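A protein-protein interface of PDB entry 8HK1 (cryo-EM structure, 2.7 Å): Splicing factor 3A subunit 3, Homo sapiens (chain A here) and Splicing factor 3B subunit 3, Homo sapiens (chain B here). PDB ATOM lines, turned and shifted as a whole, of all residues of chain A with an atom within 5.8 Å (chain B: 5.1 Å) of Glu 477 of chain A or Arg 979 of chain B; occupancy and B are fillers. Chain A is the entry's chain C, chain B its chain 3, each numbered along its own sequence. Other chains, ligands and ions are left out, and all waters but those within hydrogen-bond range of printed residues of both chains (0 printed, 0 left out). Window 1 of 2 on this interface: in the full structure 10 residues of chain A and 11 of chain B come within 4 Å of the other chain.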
ATOM      1  N   TRP A 471       7.243   7.457 -14.403  1.00  0.00           N
ATOM      2  CA  TRP A 471       8.648   7.119 -14.596  1.00  0.00           C
ATOM      3  C   TRP A 471       9.439   8.409 -14.774  1.00  0.00           C
ATOM      4  O   TRP A 471       9.355   9.052 -15.825  1.00  0.00           O
ATOM      5  CB  TRP A 471       8.826   6.204 -15.808  1.00  0.00           C
ATOM      6  CG  TRP A 471      10.220   6.191 -16.375  1.00  0.00           C
ATOM      7  CD1 TRP A 471      10.614   6.669 -17.592  1.00  0.00           C
ATOM      8  CD2 TRP A 471      11.397   5.655 -15.758  1.00  0.00           C
ATOM      9  NE1 TRP A 471      11.960   6.474 -17.764  1.00  0.00           N
ATOM     10  CE2 TRP A 471      12.467   5.857 -16.652  1.00  0.00           C
ATOM     11  CE3 TRP A 471      11.652   5.037 -14.532  1.00  0.00           C
ATOM     12  CZ2 TRP A 471      13.766   5.457 -16.362  1.00  0.00           C
ATOM     13  CZ3 TRP A 471      12.945   4.638 -14.247  1.00  0.00           C
ATOM     14  CH2 TRP A 471      13.984   4.846 -15.159  1.00  0.00           C
ATOM     15  N   GLN A 472      10.196   8.790 -13.748  1.00  0.00           N
ATOM     16  CA  GLN A 472      10.991  10.011 -13.796  1.00  0.00           C
ATOM     17  C   GLN A 472      12.455   9.665 -14.026  1.00  0.00           C
ATOM     18  O   GLN A 472      13.162   9.321 -13.067  1.00  0.00           O
ATOM     19  CB  GLN A 472      10.826  10.820 -12.507  1.00  0.00           C
ATOM     20  CG  GLN A 472      10.533   9.985 -11.275  1.00  0.00           C
ATOM     21  CD  GLN A 472       9.094  10.113 -10.819  1.00  0.00           C
ATOM     22  OE1 GLN A 472       8.515  11.200 -10.854  1.00  0.00           O
ATOM     23  NE2 GLN A 472       8.508   9.004 -10.385  1.00  0.00           N
ATOM     24  N   PRO A 473      12.955   9.760 -15.260  1.00  0.00           N
ATOM     25  CA  PRO A 473      14.321   9.286 -15.532  1.00  0.00           C
ATOM     26  C   PRO A 473      15.410  10.095 -14.844  1.00  0.00           C
ATOM     27  O   PRO A 473      16.500   9.565 -14.600  1.00  0.00           O
ATOM     28  CB  PRO A 473      14.420   9.384 -17.060  1.00  0.00           C
ATOM     29  CG  PRO A 473      13.427  10.425 -17.437  1.00  0.00           C
ATOM     30  CD  PRO A 473      12.297  10.293 -16.463  1.00  0.00           C
ATOM     31  N   ASP A 474      15.148  11.365 -14.524  1.00  0.00           N
ATOM     32  CA  ASP A 474      16.192  12.220 -13.958  1.00  0.00           C
ATOM     33  C   ASP A 474      16.704  11.670 -12.632  1.00  0.00           C
ATOM     34  O   ASP A 474      17.917  11.542 -12.427  1.00  0.00           O
ATOM     35  CB  ASP A 474      15.666  13.642 -13.775  1.00  0.00           C
ATOM     36  CG  ASP A 474      14.840  14.111 -14.953  1.00  0.00           C
ATOM     37  OD1 ASP A 474      13.635  14.386 -14.763  1.00  0.00           O
ATOM     38  OD2 ASP A 474      15.393  14.202 -16.068  1.00  0.00           O
ATOM     39  N   THR A 475      15.792  11.345 -11.712  1.00  0.00           N
ATOM     40  CA  THR A 475      16.207  10.830 -10.413  1.00  0.00           C
ATOM     41  C   THR A 475      16.220   9.304 -10.408  1.00  0.00           C
ATOM     42  O   THR A 475      16.960   8.677  -9.640  1.00  0.00           O
ATOM     43  CB  THR A 475      15.295  11.373  -9.309  1.00  0.00           C
ATOM     44  OG1 THR A 475      15.480  10.609  -8.112  1.00  0.00           O
ATOM     45  CG2 THR A 475      13.830  11.306  -9.729  1.00  0.00           C
ATOM     46  N   GLU A 476      15.413   8.692 -11.267  1.00  0.00           N
ATOM     47  CA  GLU A 476      15.377   7.245 -11.414  1.00  0.00           C
ATOM     48  C   GLU A 476      16.172   6.849 -12.648  1.00  0.00           C
ATOM     49  O   GLU A 476      15.634   6.848 -13.758  1.00  0.00           O
ATOM     50  CB  GLU A 476      13.944   6.735 -11.534  1.00  0.00           C
ATOM     51  CG  GLU A 476      13.327   6.286 -10.235  1.00  0.00           C
ATOM     52  CD  GLU A 476      11.860   5.961 -10.389  1.00  0.00           C
ATOM     53  OE1 GLU A 476      11.069   6.888 -10.660  1.00  0.00           O
ATOM     54  OE2 GLU A 476      11.494   4.777 -10.252  1.00  0.00           O
ATOM     55  N   GLU A 477      17.448   6.535 -12.447  1.00  0.00           N
ATOM     56  CA  GLU A 477      18.312   5.994 -13.490  1.00  0.00           C
ATOM     57  C   GLU A 477      19.645   5.618 -12.864  1.00  0.00           C
ATOM     58  O   GLU A 477      20.043   6.196 -11.845  1.00  0.00           O
ATOM     59  CB  GLU A 477      18.513   6.994 -14.631  1.00  0.00           C
ATOM     60  CG  GLU A 477      18.976   6.363 -15.930  1.00  0.00           C
ATOM     61  CD  GLU A 477      18.110   6.761 -17.104  1.00  0.00           C
ATOM     62  OE1 GLU A 477      18.521   6.531 -18.261  1.00  0.00           O
ATOM     63  OE2 GLU A 477      17.012   7.302 -16.867  1.00  0.00           O
ATOM     64  N   GLU A 478      20.345   4.660 -13.460  1.00  0.00           N
ATOM     65  CA  GLU A 478      21.616   4.176 -12.932  1.00  0.00           C
ATOM     66  C   GLU A 478      22.669   4.363 -14.015  1.00  0.00           C
ATOM     67  O   GLU A 478      22.745   3.577 -14.963  1.00  0.00           O
ATOM     68  CB  GLU A 478      21.514   2.720 -12.495  1.00  0.00           C
ATOM     69  N   TYR A 479      23.467   5.418 -13.884  1.00  0.00           N
ATOM     70  CA  TYR A 479      24.612   5.618 -14.755  1.00  0.00           C
ATOM     71  C   TYR A 479      25.891   5.313 -13.987  1.00  0.00           C
ATOM     72  O   TYR A 479      25.966   5.542 -12.777  1.00  0.00           O
ATOM     73  CB  TYR A 479      24.638   7.049 -15.291  1.00  0.00           C
ATOM     74  N   THR A 491      25.847   7.082  -9.639  1.00  0.00           N
ATOM     75  CA  THR A 491      25.692   8.380 -10.283  1.00  0.00           C
ATOM     76  C   THR A 491      24.275   8.533 -10.821  1.00  0.00           C
ATOM     77  O   THR A 491      23.753   7.630 -11.484  1.00  0.00           O
ATOM     78  CB  THR A 491      26.711   8.534 -11.409  1.00  0.00           C
ATOM     79  N   TYR A 492      23.652   9.673 -10.533  1.00  0.00           N
ATOM     80  CA  TYR A 492      22.346   9.998 -11.085  1.00  0.00           C
ATOM     81  C   TYR A 492      22.516  10.463 -12.531  1.00  0.00           C
ATOM     82  O   TYR A 492      23.603  10.396 -13.109  1.00  0.00           O
ATOM     83  CB  TYR A 492      21.650  11.046 -10.219  1.00  0.00           C
ATOM     84  N   GLU A 493      21.430  10.942 -13.140  1.00  0.00           N
ATOM     85  CA  GLU A 493      21.504  11.413 -14.517  1.00  0.00           C
ATOM     86  C   GLU A 493      22.095  12.814 -14.619  1.00  0.00           C
ATOM     87  O   GLU A 493      22.467  13.235 -15.718  1.00  0.00           O
ATOM     88  CB  GLU A 493      20.115  11.385 -15.158  1.00  0.00           C
ATOM     89  N   ARG B 968      11.202  -3.758 -15.773  1.00  0.00           N
ATOM     90  CA  ARG B 968      12.375  -2.901 -15.852  1.00  0.00           C
ATOM     91  C   ARG B 968      13.277  -3.332 -16.999  1.00  0.00           C
ATOM     92  O   ARG B 968      13.303  -4.497 -17.401  1.00  0.00           O
ATOM     93  CB  ARG B 968      13.164  -2.918 -14.536  1.00  0.00           C
ATOM     94  CG  ARG B 968      12.490  -2.184 -13.397  1.00  0.00           C
ATOM     95  CD  ARG B 968      13.198  -2.454 -12.090  1.00  0.00           C
ATOM     96  NE  ARG B 968      12.692  -1.620 -11.008  1.00  0.00           N
ATOM     97  CZ  ARG B 968      13.028  -1.771  -9.732  1.00  0.00           C
ATOM     98  NH1 ARG B 968      13.874  -2.728  -9.379  1.00  0.00           N
ATOM     99  NH2 ARG B 968      12.521  -0.967  -8.813  1.00  0.00           N
ATOM    100  N   VAL B 969      14.026  -2.361 -17.519  1.00  0.00           N
ATOM    101  CA  VAL B 969      15.087  -2.585 -18.493  1.00  0.00           C
ATOM    102  C   VAL B 969      16.402  -2.457 -17.735  1.00  0.00           C
ATOM    103  O   VAL B 969      16.537  -1.584 -16.871  1.00  0.00           O
ATOM    104  CB  VAL B 969      15.028  -1.592 -19.663  1.00  0.00           C
ATOM    105  CG1 VAL B 969      16.175  -1.831 -20.623  1.00  0.00           C
ATOM    106  CG2 VAL B 969      13.703  -1.704 -20.391  1.00  0.00           C
ATOM    107  N   TYR B 970      17.360  -3.319 -18.050  1.00  0.00           N
ATOM    108  CA  TYR B 970      18.632  -3.390 -17.345  1.00  0.00           C
ATOM    109  C   TYR B 970      19.775  -3.539 -18.343  1.00  0.00           C
ATOM    110  O   TYR B 970      19.734  -4.374 -19.251  1.00  0.00           O
ATOM    111  CB  TYR B 970      18.637  -4.556 -16.353  1.00  0.00           C
ATOM    112  CG  TYR B 970      18.122  -4.224 -14.977  1.00  0.00           C
ATOM    113  CD1 TYR B 970      18.861  -3.432 -14.113  1.00  0.00           C
ATOM    114  CD2 TYR B 970      16.900  -4.712 -14.536  1.00  0.00           C
ATOM    115  CE1 TYR B 970      18.396  -3.131 -12.851  1.00  0.00           C
ATOM    116  CE2 TYR B 970      16.427  -4.416 -13.276  1.00  0.00           C
ATOM    117  CZ  TYR B 970      17.179  -3.624 -12.438  1.00  0.00           C
ATOM    118  OH  TYR B 970      16.712  -3.328 -11.182  1.00  0.00           O
ATOM    119  N   LEU B 977      23.917  -4.293 -12.268  1.00  0.00           N
ATOM    120  CA  LEU B 977      23.060  -4.010 -13.407  1.00  0.00           C
ATOM    121  C   LEU B 977      22.404  -2.645 -13.240  1.00  0.00           C
ATOM    122  O   LEU B 977      21.933  -2.283 -12.159  1.00  0.00           O
ATOM    123  CB  LEU B 977      21.993  -5.095 -13.572  1.00  0.00           C
ATOM    124  CG  LEU B 977      22.492  -6.512 -13.857  1.00  0.00           C
ATOM    125  CD1 LEU B 977      21.372  -7.510 -13.678  1.00  0.00           C
ATOM    126  CD2 LEU B 977      23.068  -6.605 -15.258  1.00  0.00           C
ATOM    127  N   LEU B 978      22.382  -1.888 -14.329  1.00  0.00           N
ATOM    128  CA  LEU B 978      21.970  -0.486 -14.317  1.00  0.00           C
ATOM    129  C   LEU B 978      20.535  -0.391 -14.823  1.00  0.00           C
ATOM    130  O   LEU B 978      20.240  -0.783 -15.956  1.00  0.00           O
ATOM    131  CB  LEU B 978      22.917   0.355 -15.163  1.00  0.00           C
ATOM    132  CG  LEU B 978      24.388   0.283 -14.754  1.00  0.00           C
ATOM    133  CD1 LEU B 978      25.264   0.943 -15.799  1.00  0.00           C
ATOM    134  CD2 LEU B 978      24.603   0.918 -13.393  1.00  0.00           C
ATOM    135  N   ARG B 979      19.645   0.129 -13.983  1.00  0.00           N
ATOM    136  CA  ARG B 979      18.252   0.318 -14.367  1.00  0.00           C
ATOM    137  C   ARG B 979      18.147   1.442 -15.389  1.00  0.00           C
ATOM    138  O   ARG B 979      18.722   2.518 -15.204  1.00  0.00           O
ATOM    139  CB  ARG B 979      17.406   0.628 -13.137  1.00  0.00           C
ATOM    140  CG  ARG B 979      15.938   0.849 -13.442  1.00  0.00           C
ATOM    141  CD  ARG B 979      15.081   0.630 -12.212  1.00  0.00           C
ATOM    142  NE  ARG B 979      14.893   1.850 -11.437  1.00  0.00           N
ATOM    143  CZ  ARG B 979      15.466   2.084 -10.262  1.00  0.00           C
ATOM    144  NH1 ARG B 979      16.270   1.177  -9.721  1.00  0.00           N
ATOM    145  NH2 ARG B 979      15.233   3.221  -9.625  1.00  0.00           N
ATOM    146  N   LYS B 980      17.403   1.197 -16.467  1.00  0.00           N
ATOM    147  CA  LYS B 980      17.335   2.116 -17.595  1.00  0.00           C
ATOM    148  C   LYS B 980      15.925   2.634 -17.855  1.00  0.00           C
ATOM    149  O   LYS B 980      15.750   3.802 -18.203  1.00  0.00           O
ATOM    150  CB  LYS B 980      17.880   1.436 -18.854  1.00  0.00           C
ATOM    151  CG  LYS B 980      19.389   1.297 -18.869  1.00  0.00           C
ATOM    152  CD  LYS B 980      20.060   2.651 -18.998  1.00  0.00           C
ATOM    153  CE  LYS B 980      21.566   2.526 -18.929  1.00  0.00           C
ATOM    154  NZ  LYS B 980      22.065   2.618 -17.536  1.00  0.00           N
ATOM    155  N   CYS B 981      14.916   1.781 -17.704  1.00  0.00           N
ATOM    156  CA  CYS B 981      13.531   2.167 -17.917  1.00  0.00           C
ATOM    157  C   CYS B 981      12.648   1.336 -17.001  1.00  0.00           C
ATOM    158  O   CYS B 981      13.067   0.303 -16.478  1.00  0.00           O
ATOM    159  CB  CYS B 981      13.111   1.985 -19.382  1.00  0.00           C
ATOM    160  SG  CYS B 981      11.640   2.909 -19.864  1.00  0.00           S
ATOM    161  N   GLU B 982      11.412   1.795 -16.815  1.00  0.00           N
ATOM    162  CA  GLU B 982      10.520   1.137 -15.869  1.00  0.00           C
ATOM    163  C   GLU B 982       9.074   1.492 -16.178  1.00  0.00           C
ATOM    164  O   GLU B 982       8.760   2.656 -16.438  1.00  0.00           O
ATOM    165  CB  GLU B 982      10.869   1.536 -14.433  1.00  0.00           C
ATOM    166  CG  GLU B 982       9.892   1.037 -13.392  1.00  0.00           C
ATOM    167  CD  GLU B 982      10.425   1.182 -11.983  1.00  0.00           C
ATOM    168  OE1 GLU B 982      11.450   1.870 -11.801  1.00  0.00           O
ATOM    169  OE2 GLU B 982       9.815   0.620 -11.054  1.00  0.00           O
ATOM    170  N   ASN B1019      12.736   6.347 -24.589  1.00  0.00           N
ATOM    171  CA  ASN B1019      13.051   5.553 -23.401  1.00  0.00           C
ATOM    172  C   ASN B1019      11.811   5.397 -22.512  1.00  0.00           C
ATOM    173  O   ASN B1019      11.784   5.790 -21.344  1.00  0.00           O
ATOM    174  CB  ASN B1019      14.220   6.173 -22.626  1.00  0.00           C
ATOM    175  CG  ASN B1019      14.942   5.168 -21.757  1.00  0.00           C
ATOM    176  OD1 ASN B1019      15.311   4.086 -22.212  1.00  0.00           O
ATOM    177  ND2 ASN B1019      15.147   5.517 -20.495  1.00  0.00           N
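The backbone NH of Glu 478 of chain A lies within hydrogen-bond range of the backbone carbonyl oxygen of Arg 979 of chain B, at 3.2 Å.
The backbone carbonyl oxygen of Glu 478 of chain A sits at hydrogen-bond distance from the side-chain amino group of Lys 980 of chain B, at 2.8 Å.
The side-chain carboxylate (OE2) of Glu 476 of chain A sits close to the side-chain carboxylate (OE1) of Glu 982 of chain B, at 3.3 Å.
The backbone carbonyl oxygen of Val 969 of chain B lies within hydrogen-bond range of the backbone NH of Lys 980 of chain B.
The backbone carbonyl oxygen (O) of Cys 981 of chain B sits at hydrogen-bond distance from the backbone NH (N) of Val 969 of chain B (3.0 Å).
The side-chain carboxylate of Glu 476 of chain A sits close to the side-chain amide nitrogen of Gln 472 of chain A, 3.3 Å away.
The guanidinium group (NE) of Arg 968 of chain B lies within salt-bridge range of the side-chain carboxylate (OE2) of Glu 982 of chain B (3.6 Å).
NE of Arg 979 of chain B is in salt-bridge range of OE1 of Glu 982 of chain B, 3.5 Å away.
The side-chain amide nitrogen (ND2) of Asn 1019 of chain B is in hydrogen-bond range of the backbone carbonyl oxygen (O) of Lys 980 of chain B (2.9 Å).
Among the printed residues, pairs that only touch across the chains: Trp 471 of chain A with Lys 980 of chain B (3.2 Å), Trp 471 of chain A with Cys 981 of chain B (3.6 Å), Trp 471 of chain A with Glu 982 of chain B (3.6 Å), Trp 471 of chain A with Asn 1019 of chain B (3.6 Å), Glu 476 of chain A with Arg 979 of chain B (3.7 Å), Glu 477 of chain A with Arg 979 of chain B (3.9 Å), Glu 477 of chain A with Lys 980 of chain B (3.9 Å) and Glu 478 of chain A with Leu 978 of chain B (3.2 Å).
Of the printed residues of chain B, Trp 471 of chain A touches Lys 980, Cys 981, Glu 982 and Asn 1019.
Of the printed residues of chain B, Glu 476 of chain A touches Arg 979 (3.7 Å) and Glu 982 (3.3 Å).
Of the printed residues of chain B, Glu 477 of chain A touches Arg 979 and Lys 980.
Tyr 479 of chain A touches none of the printed residues of chain B.
Thr 491 of chain A touches none of the printed residues of chain B.
Arg 979 of chain B touches just these residues of chain A: Glu 476 (3.7 Å), Glu 477 (3.9 Å) and Glu 478 (3.2 Å).
The nearest residue of chain B that does not touch Glu 477 of chain A is Asn 1019 of chain B (4.2 Å).
The nearest printed residue of chain A that does not touch Glu 982 of chain B is Gln 472 of chain A (6.9 Å).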
